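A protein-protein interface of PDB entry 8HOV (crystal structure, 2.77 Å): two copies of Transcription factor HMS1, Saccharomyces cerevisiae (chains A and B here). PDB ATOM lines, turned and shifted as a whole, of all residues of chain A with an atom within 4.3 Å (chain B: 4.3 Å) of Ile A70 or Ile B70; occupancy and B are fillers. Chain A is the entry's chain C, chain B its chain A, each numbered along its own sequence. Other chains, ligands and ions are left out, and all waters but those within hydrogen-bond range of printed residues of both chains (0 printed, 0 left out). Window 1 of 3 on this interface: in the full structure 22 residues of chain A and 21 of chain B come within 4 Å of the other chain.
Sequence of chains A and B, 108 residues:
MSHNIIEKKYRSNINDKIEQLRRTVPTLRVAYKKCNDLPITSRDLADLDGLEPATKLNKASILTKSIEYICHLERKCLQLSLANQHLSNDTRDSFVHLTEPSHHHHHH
The side-chain hydroxyl (OH) of Tyr B69 sits at hydrogen-bond distance from the side-chain carboxylate (OE2) of Glu A74 (2.7 Å). The side-chain hydroxyl (OH) of Tyr A69 lies within hydrogen-bond range of the side-chain carboxylate (OE2) of Glu B74 (2.7 Å).
Leu A21 touches Ile B67, and with the chains exchanged Ile A67 touches Leu B21. Leu A21 touches Ile B70, and with the chains exchanged Ile A70 touches Leu B21. Thr A24 touches Ile B70, and with the chains exchanged Ile A70 touches Thr B24. Leu A73 touches its own counterpart, Leu B73. Positions printed for both chains: 21, 24, 66, 67, 68, 69, 70, 71, 72, 73 and 74.
Of the printed residues of chain B, Leu A21 touches Ile B67 (3.7 Å) and Ile B70 (3.9 Å). Printed residues of chain A within 4 Å of Tyr B69: Ile A70 and Glu A74. Ile B70 touches just these residues of chain A: Leu A21 (3.9 Å), Thr A24 (3.7 Å), Tyr A69 (3.7 Å), Ile A70 (3.6 Å) and Leu A73 (3.9 Å). Printed residues of chain A within 4 Å of Leu B73: Ile A70 (3.9 Å), Leu A73 (3.9 Å) and Glu A74 (3.7 Å). Of the printed residues of chain A, Glu B74 touches Tyr A69 and Leu A73. The nearest printed residue of chain B that does not touch Ile A70 is Ser B66 (4.5 Å). The nearest printed residue of chain A that does not touch Ile B70 is Ser A66 (4.6 Å).
Of the 11 printed residues of chain B, 7 touch a printed residue of chain A. Hydrophobic or aromatic side chains of chain B that line the printed part of chain A: Leu B21, Ile B67, Tyr B69, Ile B70 and Leu B73. Among the printed residues, no Asp or Glu carboxylate lies within 4 Å of a Lys or Arg side-chain nitrogen of the other chain.
Among the printed residues, pairs that only touch across the chains: Ile A70 with Ile B70 (3.6 Å), Leu A73 with Glu B74 (3.6 Å), Ile A70 with Tyr B69 (3.6 Å), Ile A67 with Leu B21 (3.6 Å), Glu A74 with Leu B73 (3.7 Å), Tyr A69 with Ile B70 (3.7 Å), Thr A24 with Ile B70 (3.7 Å), Leu A21 with Ile B67 (3.7 Å), Ile A70 with Leu B21 (3.8 Å), Leu A73 with Ile B70 (3.9 Å), Ile A70 with Thr B24 (3.9 Å), Leu A21 with Ile B70 (3.9 Å), Leu A73 with Leu B73 (3.9 Å) and Ile A70 with Leu B73 (3.9 Å).
O of Ile B67 is in hydrogen-bond range of SG of Cys B71, 3.4 Å away. The backbone carbonyl oxygen of Ile A67 is in hydrogen-bond range of the side-chain sulfur of Cys A71 (3.5 Å).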
ATOM      1  N   LEU A  21     -21.298 -14.525  -1.615  1.00  0.00           N
ATOM      2  CA  LEU A  21     -20.368 -15.383  -2.344  1.00  0.00           C
ATOM      3  C   LEU A  21     -20.040 -16.639  -1.547  1.00  0.00           C
ATOM      4  O   LEU A  21     -19.902 -17.727  -2.116  1.00  0.00           O
ATOM      5  CB  LEU A  21     -19.092 -14.611  -2.678  1.00  0.00           C
ATOM      6  CG  LEU A  21     -19.197 -13.507  -3.730  1.00  0.00           C
ATOM      7  CD1 LEU A  21     -17.955 -12.632  -3.710  1.00  0.00           C
ATOM      8  CD2 LEU A  21     -19.400 -14.113  -5.109  1.00  0.00           C
ATOM      9  N   THR A  24     -22.800 -18.955  -1.991  1.00  0.00           N
ATOM     10  CA  THR A  24     -23.043 -19.313  -3.383  1.00  0.00           C
ATOM     11  C   THR A  24     -21.999 -20.269  -3.940  1.00  0.00           C
ATOM     12  O   THR A  24     -22.353 -21.270  -4.571  1.00  0.00           O
ATOM     13  CB  THR A  24     -23.098 -18.045  -4.250  1.00  0.00           C
ATOM     14  OG1 THR A  24     -24.159 -17.198  -3.792  1.00  0.00           O
ATOM     15  CG2 THR A  24     -23.336 -18.404  -5.708  1.00  0.00           C
ATOM     16  N   SER A  66     -14.250 -17.592  -5.547  1.00  0.00           N
ATOM     17  CA  SER A  66     -15.253 -17.084  -6.479  1.00  0.00           C
ATOM     18  C   SER A  66     -14.684 -16.961  -7.886  1.00  0.00           C
ATOM     19  O   SER A  66     -15.360 -17.289  -8.868  1.00  0.00           O
ATOM     20  CB  SER A  66     -15.789 -15.738  -5.995  1.00  0.00           C
ATOM     21  OG  SER A  66     -16.483 -15.878  -4.766  1.00  0.00           O
ATOM     22  N   ILE A  67     -13.441 -16.488  -8.006  1.00  0.00           N
ATOM     23  CA  ILE A  67     -12.779 -16.456  -9.306  1.00  0.00           C
ATOM     24  C   ILE A  67     -12.610 -17.869  -9.848  1.00  0.00           C
ATOM     25  O   ILE A  67     -12.797 -18.120 -11.044  1.00  0.00           O
ATOM     26  CB  ILE A  67     -11.429 -15.723  -9.203  1.00  0.00           C
ATOM     27  CG1 ILE A  67     -11.632 -14.295  -8.697  1.00  0.00           C
ATOM     28  CG2 ILE A  67     -10.717 -15.719 -10.550  1.00  0.00           C
ATOM     29  CD1 ILE A  67     -10.345 -13.554  -8.422  1.00  0.00           C
ATOM     30  N   GLU A  68     -12.245 -18.810  -8.973  1.00  0.00           N
ATOM     31  CA  GLU A  68     -12.087 -20.202  -9.386  1.00  0.00           C
ATOM     32  C   GLU A  68     -13.402 -20.779  -9.893  1.00  0.00           C
ATOM     33  O   GLU A  68     -13.438 -21.472 -10.918  1.00  0.00           O
ATOM     34  CB  GLU A  68     -11.550 -21.030  -8.216  1.00  0.00           C
ATOM     35  CG  GLU A  68     -11.534 -22.528  -8.459  1.00  0.00           C
ATOM     36  CD  GLU A  68     -11.691 -23.325  -7.175  1.00  0.00           C
ATOM     37  OE1 GLU A  68     -12.678 -23.086  -6.445  1.00  0.00           O
ATOM     38  OE2 GLU A  68     -10.828 -24.183  -6.891  1.00  0.00           O
ATOM     39  N   TYR A  69     -14.499 -20.507  -9.183  1.00  0.00           N
ATOM     40  CA  TYR A  69     -15.791 -21.070  -9.563  1.00  0.00           C
ATOM     41  C   TYR A  69     -16.295 -20.478 -10.875  1.00  0.00           C
ATOM     42  O   TYR A  69     -16.922 -21.181 -11.677  1.00  0.00           O
ATOM     43  CB  TYR A  69     -16.805 -20.846  -8.442  1.00  0.00           C
ATOM     44  CG  TYR A  69     -18.100 -21.604  -8.621  1.00  0.00           C
ATOM     45  CD1 TYR A  69     -18.098 -22.948  -8.968  1.00  0.00           C
ATOM     46  CD2 TYR A  69     -19.325 -20.980  -8.424  1.00  0.00           C
ATOM     47  CE1 TYR A  69     -19.279 -23.647  -9.127  1.00  0.00           C
ATOM     48  CE2 TYR A  69     -20.512 -21.671  -8.579  1.00  0.00           C
ATOM     49  CZ  TYR A  69     -20.483 -23.003  -8.931  1.00  0.00           C
ATOM     50  OH  TYR A  69     -21.661 -23.693  -9.086  1.00  0.00           O
ATOM     51  N   ILE A  70     -16.037 -19.189 -11.106  1.00  0.00           N
ATOM     52  CA  ILE A  70     -16.473 -18.548 -12.345  1.00  0.00           C
ATOM     53  C   ILE A  70     -15.788 -19.190 -13.546  1.00  0.00           C
ATOM     54  O   ILE A  70     -16.436 -19.545 -14.537  1.00  0.00           O
ATOM     55  CB  ILE A  70     -16.206 -17.034 -12.284  1.00  0.00           C
ATOM     56  CG1 ILE A  70     -17.187 -16.357 -11.325  1.00  0.00           C
ATOM     57  CG2 ILE A  70     -16.296 -16.414 -13.668  1.00  0.00           C
ATOM     58  CD1 ILE A  70     -16.925 -14.883 -11.124  1.00  0.00           C
ATOM     59  N   CYS A  71     -14.483 -19.393 -13.477  1.00  0.00           N
ATOM     60  CA  CYS A  71     -13.772 -19.949 -14.653  1.00  0.00           C
ATOM     61  C   CYS A  71     -14.220 -21.396 -14.868  1.00  0.00           C
ATOM     62  O   CYS A  71     -14.420 -21.803 -16.036  1.00  0.00           O
ATOM     63  CB  CYS A  71     -12.266 -19.880 -14.443  1.00  0.00           C
ATOM     64  SG  CYS A  71     -11.635 -18.185 -14.364  1.00  0.00           S
ATOM     65  N   HIS A  72     -14.394 -22.134 -13.776  1.00  0.00           N
ATOM     66  CA  HIS A  72     -14.834 -23.547 -13.866  1.00  0.00           C
ATOM     67  C   HIS A  72     -16.199 -23.611 -14.543  1.00  0.00           C
ATOM     68  O   HIS A  72     -16.345 -24.390 -15.494  1.00  0.00           O
ATOM     69  CB  HIS A  72     -14.868 -24.163 -12.468  1.00  0.00           C
ATOM     70  CG  HIS A  72     -15.525 -25.497 -12.386  1.00  0.00           C
ATOM     71  ND1 HIS A  72     -14.876 -26.661 -12.733  1.00  0.00           N
ATOM     72  CD2 HIS A  72     -16.756 -25.858 -11.968  1.00  0.00           C
ATOM     73  CE1 HIS A  72     -15.687 -27.683 -12.551  1.00  0.00           C
ATOM     74  NE2 HIS A  72     -16.845 -27.215 -12.082  1.00  0.00           N
ATOM     75  N   LEU A  73     -17.147 -22.809 -14.069  1.00  0.00           N
ATOM     76  CA  LEU A  73     -18.511 -22.840 -14.641  1.00  0.00           C
ATOM     77  C   LEU A  73     -18.413 -22.487 -16.124  1.00  0.00           C
ATOM     78  O   LEU A  73     -19.100 -23.119 -16.918  1.00  0.00           O
ATOM     79  CB  LEU A  73     -19.394 -21.846 -13.888  1.00  0.00           C
ATOM     80  CG  LEU A  73     -19.954 -22.326 -12.553  1.00  0.00           C
ATOM     81  CD1 LEU A  73     -20.819 -21.246 -11.928  1.00  0.00           C
ATOM     82  CD2 LEU A  73     -20.756 -23.602 -12.738  1.00  0.00           C
ATOM     83  N   GLU A  74     -17.556 -21.532 -16.472  1.00  0.00           N
ATOM     84  CA  GLU A  74     -17.413 -21.105 -17.884  1.00  0.00           C
ATOM     85  C   GLU A  74     -16.968 -22.298 -18.717  1.00  0.00           C
ATOM     86  O   GLU A  74     -17.621 -22.595 -19.720  1.00  0.00           O
ATOM     87  CB  GLU A  74     -16.378 -19.988 -18.008  1.00  0.00           C
ATOM     88  CG  GLU A  74     -16.861 -18.640 -17.511  1.00  0.00           C
ATOM     89  CD  GLU A  74     -15.837 -17.530 -17.670  1.00  0.00           C
ATOM     90  OE1 GLU A  74     -14.652 -17.850 -17.881  1.00  0.00           O
ATOM     91  OE2 GLU A  74     -16.227 -16.351 -17.592  1.00  0.00           O
ATOM     92  N   LEU B  21     -11.790  -9.823 -10.925  1.00  0.00           N
ATOM     93  CA  LEU B  21     -13.193 -10.050 -11.263  1.00  0.00           C
ATOM     94  C   LEU B  21     -13.669  -9.070 -12.328  1.00  0.00           C
ATOM     95  O   LEU B  21     -14.429  -9.442 -13.229  1.00  0.00           O
ATOM     96  CB  LEU B  21     -14.059  -9.941 -10.007  1.00  0.00           C
ATOM     97  CG  LEU B  21     -13.952 -11.081  -8.993  1.00  0.00           C
ATOM     98  CD1 LEU B  21     -14.599 -10.689  -7.672  1.00  0.00           C
ATOM     99  CD2 LEU B  21     -14.591 -12.343  -9.548  1.00  0.00           C
ATOM    100  N   THR B  24     -12.884 -10.304 -15.675  1.00  0.00           N
ATOM    101  CA  THR B  24     -13.457 -11.593 -16.044  1.00  0.00           C
ATOM    102  C   THR B  24     -14.948 -11.513 -16.330  1.00  0.00           C
ATOM    103  O   THR B  24     -15.406 -12.048 -17.346  1.00  0.00           O
ATOM    104  CB  THR B  24     -13.191 -12.625 -14.933  1.00  0.00           C
ATOM    105  OG1 THR B  24     -11.779 -12.775 -14.748  1.00  0.00           O
ATOM    106  CG2 THR B  24     -13.794 -13.973 -15.298  1.00  0.00           C
ATOM    107  N   SER B  66     -20.660  -9.840 -10.174  1.00  0.00           N
ATOM    108  CA  SER B  66     -20.034 -11.159 -10.145  1.00  0.00           C
ATOM    109  C   SER B  66     -20.997 -12.214  -9.615  1.00  0.00           C
ATOM    110  O   SER B  66     -21.045 -13.335 -10.134  1.00  0.00           O
ATOM    111  CB  SER B  66     -18.762 -11.120  -9.301  1.00  0.00           C
ATOM    112  OG  SER B  66     -17.773 -10.304  -9.901  1.00  0.00           O
ATOM    113  N   ILE B  67     -21.769 -11.875  -8.579  1.00  0.00           N
ATOM    114  CA  ILE B  67     -22.803 -12.783  -8.088  1.00  0.00           C
ATOM    115  C   ILE B  67     -23.838 -13.038  -9.176  1.00  0.00           C
ATOM    116  O   ILE B  67     -24.313 -14.168  -9.353  1.00  0.00           O
ATOM    117  CB  ILE B  67     -23.449 -12.213  -6.811  1.00  0.00           C
ATOM    118  CG1 ILE B  67     -22.389 -11.974  -5.736  1.00  0.00           C
ATOM    119  CG2 ILE B  67     -24.530 -13.149  -6.291  1.00  0.00           C
ATOM    120  CD1 ILE B  67     -22.917 -11.280  -4.502  1.00  0.00           C
ATOM    121  N   GLU B  68     -24.203 -11.993  -9.921  1.00  0.00           N
ATOM    122  CA  GLU B  68     -25.124 -12.149 -11.042  1.00  0.00           C
ATOM    123  C   GLU B  68     -24.549 -13.079 -12.103  1.00  0.00           C
ATOM    124  O   GLU B  68     -25.265 -13.917 -12.663  1.00  0.00           O
ATOM    125  CB  GLU B  68     -25.439 -10.777 -11.640  1.00  0.00           C
ATOM    126  CG  GLU B  68     -26.161 -10.810 -12.975  1.00  0.00           C
ATOM    127  CD  GLU B  68     -25.740  -9.668 -13.884  1.00  0.00           C
ATOM    128  OE1 GLU B  68     -24.535  -9.339 -13.905  1.00  0.00           O
ATOM    129  OE2 GLU B  68     -26.613  -9.098 -14.572  1.00  0.00           O
ATOM    130  N   TYR B  69     -23.253 -12.944 -12.395  1.00  0.00           N
ATOM    131  CA  TYR B  69     -22.631 -13.776 -13.418  1.00  0.00           C
ATOM    132  C   TYR B  69     -22.547 -15.235 -12.988  1.00  0.00           C
ATOM    133  O   TYR B  69     -22.672 -16.135 -13.828  1.00  0.00           O
ATOM    134  CB  TYR B  69     -21.244 -13.230 -13.755  1.00  0.00           C
ATOM    135  CG  TYR B  69     -20.587 -13.892 -14.943  1.00  0.00           C
ATOM    136  CD1 TYR B  69     -21.288 -14.099 -16.125  1.00  0.00           C
ATOM    137  CD2 TYR B  69     -19.259 -14.292 -14.891  1.00  0.00           C
ATOM    138  CE1 TYR B  69     -20.688 -14.700 -17.216  1.00  0.00           C
ATOM    139  CE2 TYR B  69     -18.651 -14.891 -15.976  1.00  0.00           C
ATOM    140  CZ  TYR B  69     -19.368 -15.092 -17.135  1.00  0.00           C
ATOM    141  OH  TYR B  69     -18.759 -15.689 -18.216  1.00  0.00           O
ATOM    142  N   ILE B  70     -22.331 -15.491 -11.695  1.00  0.00           N
ATOM    143  CA  ILE B  70     -22.271 -16.866 -11.207  1.00  0.00           C
ATOM    144  C   ILE B  70     -23.623 -17.549 -11.367  1.00  0.00           C
ATOM    145  O   ILE B  70     -23.709 -18.695 -11.825  1.00  0.00           O
ATOM    146  CB  ILE B  70     -21.799 -16.895  -9.742  1.00  0.00           C
ATOM    147  CG1 ILE B  70     -20.350 -16.422  -9.631  1.00  0.00           C
ATOM    148  CG2 ILE B  70     -21.946 -18.294  -9.166  1.00  0.00           C
ATOM    149  CD1 ILE B  70     -19.818 -16.418  -8.213  1.00  0.00           C
ATOM    150  N   CYS B  71     -24.701 -16.857 -10.990  1.00  0.00           N
ATOM    151  CA  CYS B  71     -26.035 -17.436 -11.118  1.00  0.00           C
ATOM    152  C   CYS B  71     -26.411 -17.634 -12.580  1.00  0.00           C
ATOM    153  O   CYS B  71     -27.069 -18.621 -12.928  1.00  0.00           O
ATOM    154  CB  CYS B  71     -27.063 -16.554 -10.411  1.00  0.00           C
ATOM    155  SG  CYS B  71     -26.773 -16.331  -8.641  1.00  0.00           S
ATOM    156  N   HIS B  72     -25.987 -16.740 -13.464  1.00  0.00           N
ATOM    157  CA  HIS B  72     -26.263 -16.937 -14.913  1.00  0.00           C
ATOM    158  C   HIS B  72     -25.604 -18.225 -15.408  1.00  0.00           C
ATOM    159  O   HIS B  72     -26.303 -19.041 -16.018  1.00  0.00           O
ATOM    160  CB  HIS B  72     -25.808 -15.715 -15.716  1.00  0.00           C
ATOM    161  CG  HIS B  72     -25.795 -15.909 -17.194  1.00  0.00           C
ATOM    162  ND1 HIS B  72     -26.887 -15.623 -17.983  1.00  0.00           N
ATOM    163  CD2 HIS B  72     -24.824 -16.332 -18.028  1.00  0.00           C
ATOM    164  CE1 HIS B  72     -26.593 -15.874 -19.242  1.00  0.00           C
ATOM    165  NE2 HIS B  72     -25.333 -16.311 -19.296  1.00  0.00           N
ATOM    166  N   LEU B  73     -24.310 -18.391 -15.153  1.00  0.00           N
ATOM    167  CA  LEU B  73     -23.565 -19.578 -15.643  1.00  0.00           C
ATOM    168  C   LEU B  73     -24.120 -20.853 -15.002  1.00  0.00           C
ATOM    169  O   LEU B  73     -24.110 -21.895 -15.668  1.00  0.00           O
ATOM    170  CB  LEU B  73     -22.085 -19.382 -15.310  1.00  0.00           C
ATOM    171  CG  LEU B  73     -21.348 -18.314 -16.112  1.00  0.00           C
ATOM    172  CD1 LEU B  73     -19.949 -18.109 -15.557  1.00  0.00           C
ATOM    173  CD2 LEU B  73     -21.281 -18.701 -17.579  1.00  0.00           C
ATOM    174  N   GLU B  74     -24.581 -20.770 -13.757  1.00  0.00           N
ATOM    175  CA  GLU B  74     -25.179 -21.943 -13.067  1.00  0.00           C
ATOM    176  C   GLU B  74     -26.483 -22.332 -13.764  1.00  0.00           C
ATOM    177  O   GLU B  74     -26.705 -23.533 -13.962  1.00  0.00           O
ATOM    178  CB  GLU B  74     -25.426 -21.612 -11.596  1.00  0.00           C
ATOM    179  CG  GLU B  74     -24.197 -21.743 -10.720  1.00  0.00           C
ATOM    180  CD  GLU B  74     -24.489 -21.592  -9.239  1.00  0.00           C
ATOM    181  OE1 GLU B  74     -25.620 -21.202  -8.903  1.00  0.00           O
ATOM    182  OE2 GLU B  74     -23.590 -21.874  -8.427  1.00  0.00           O
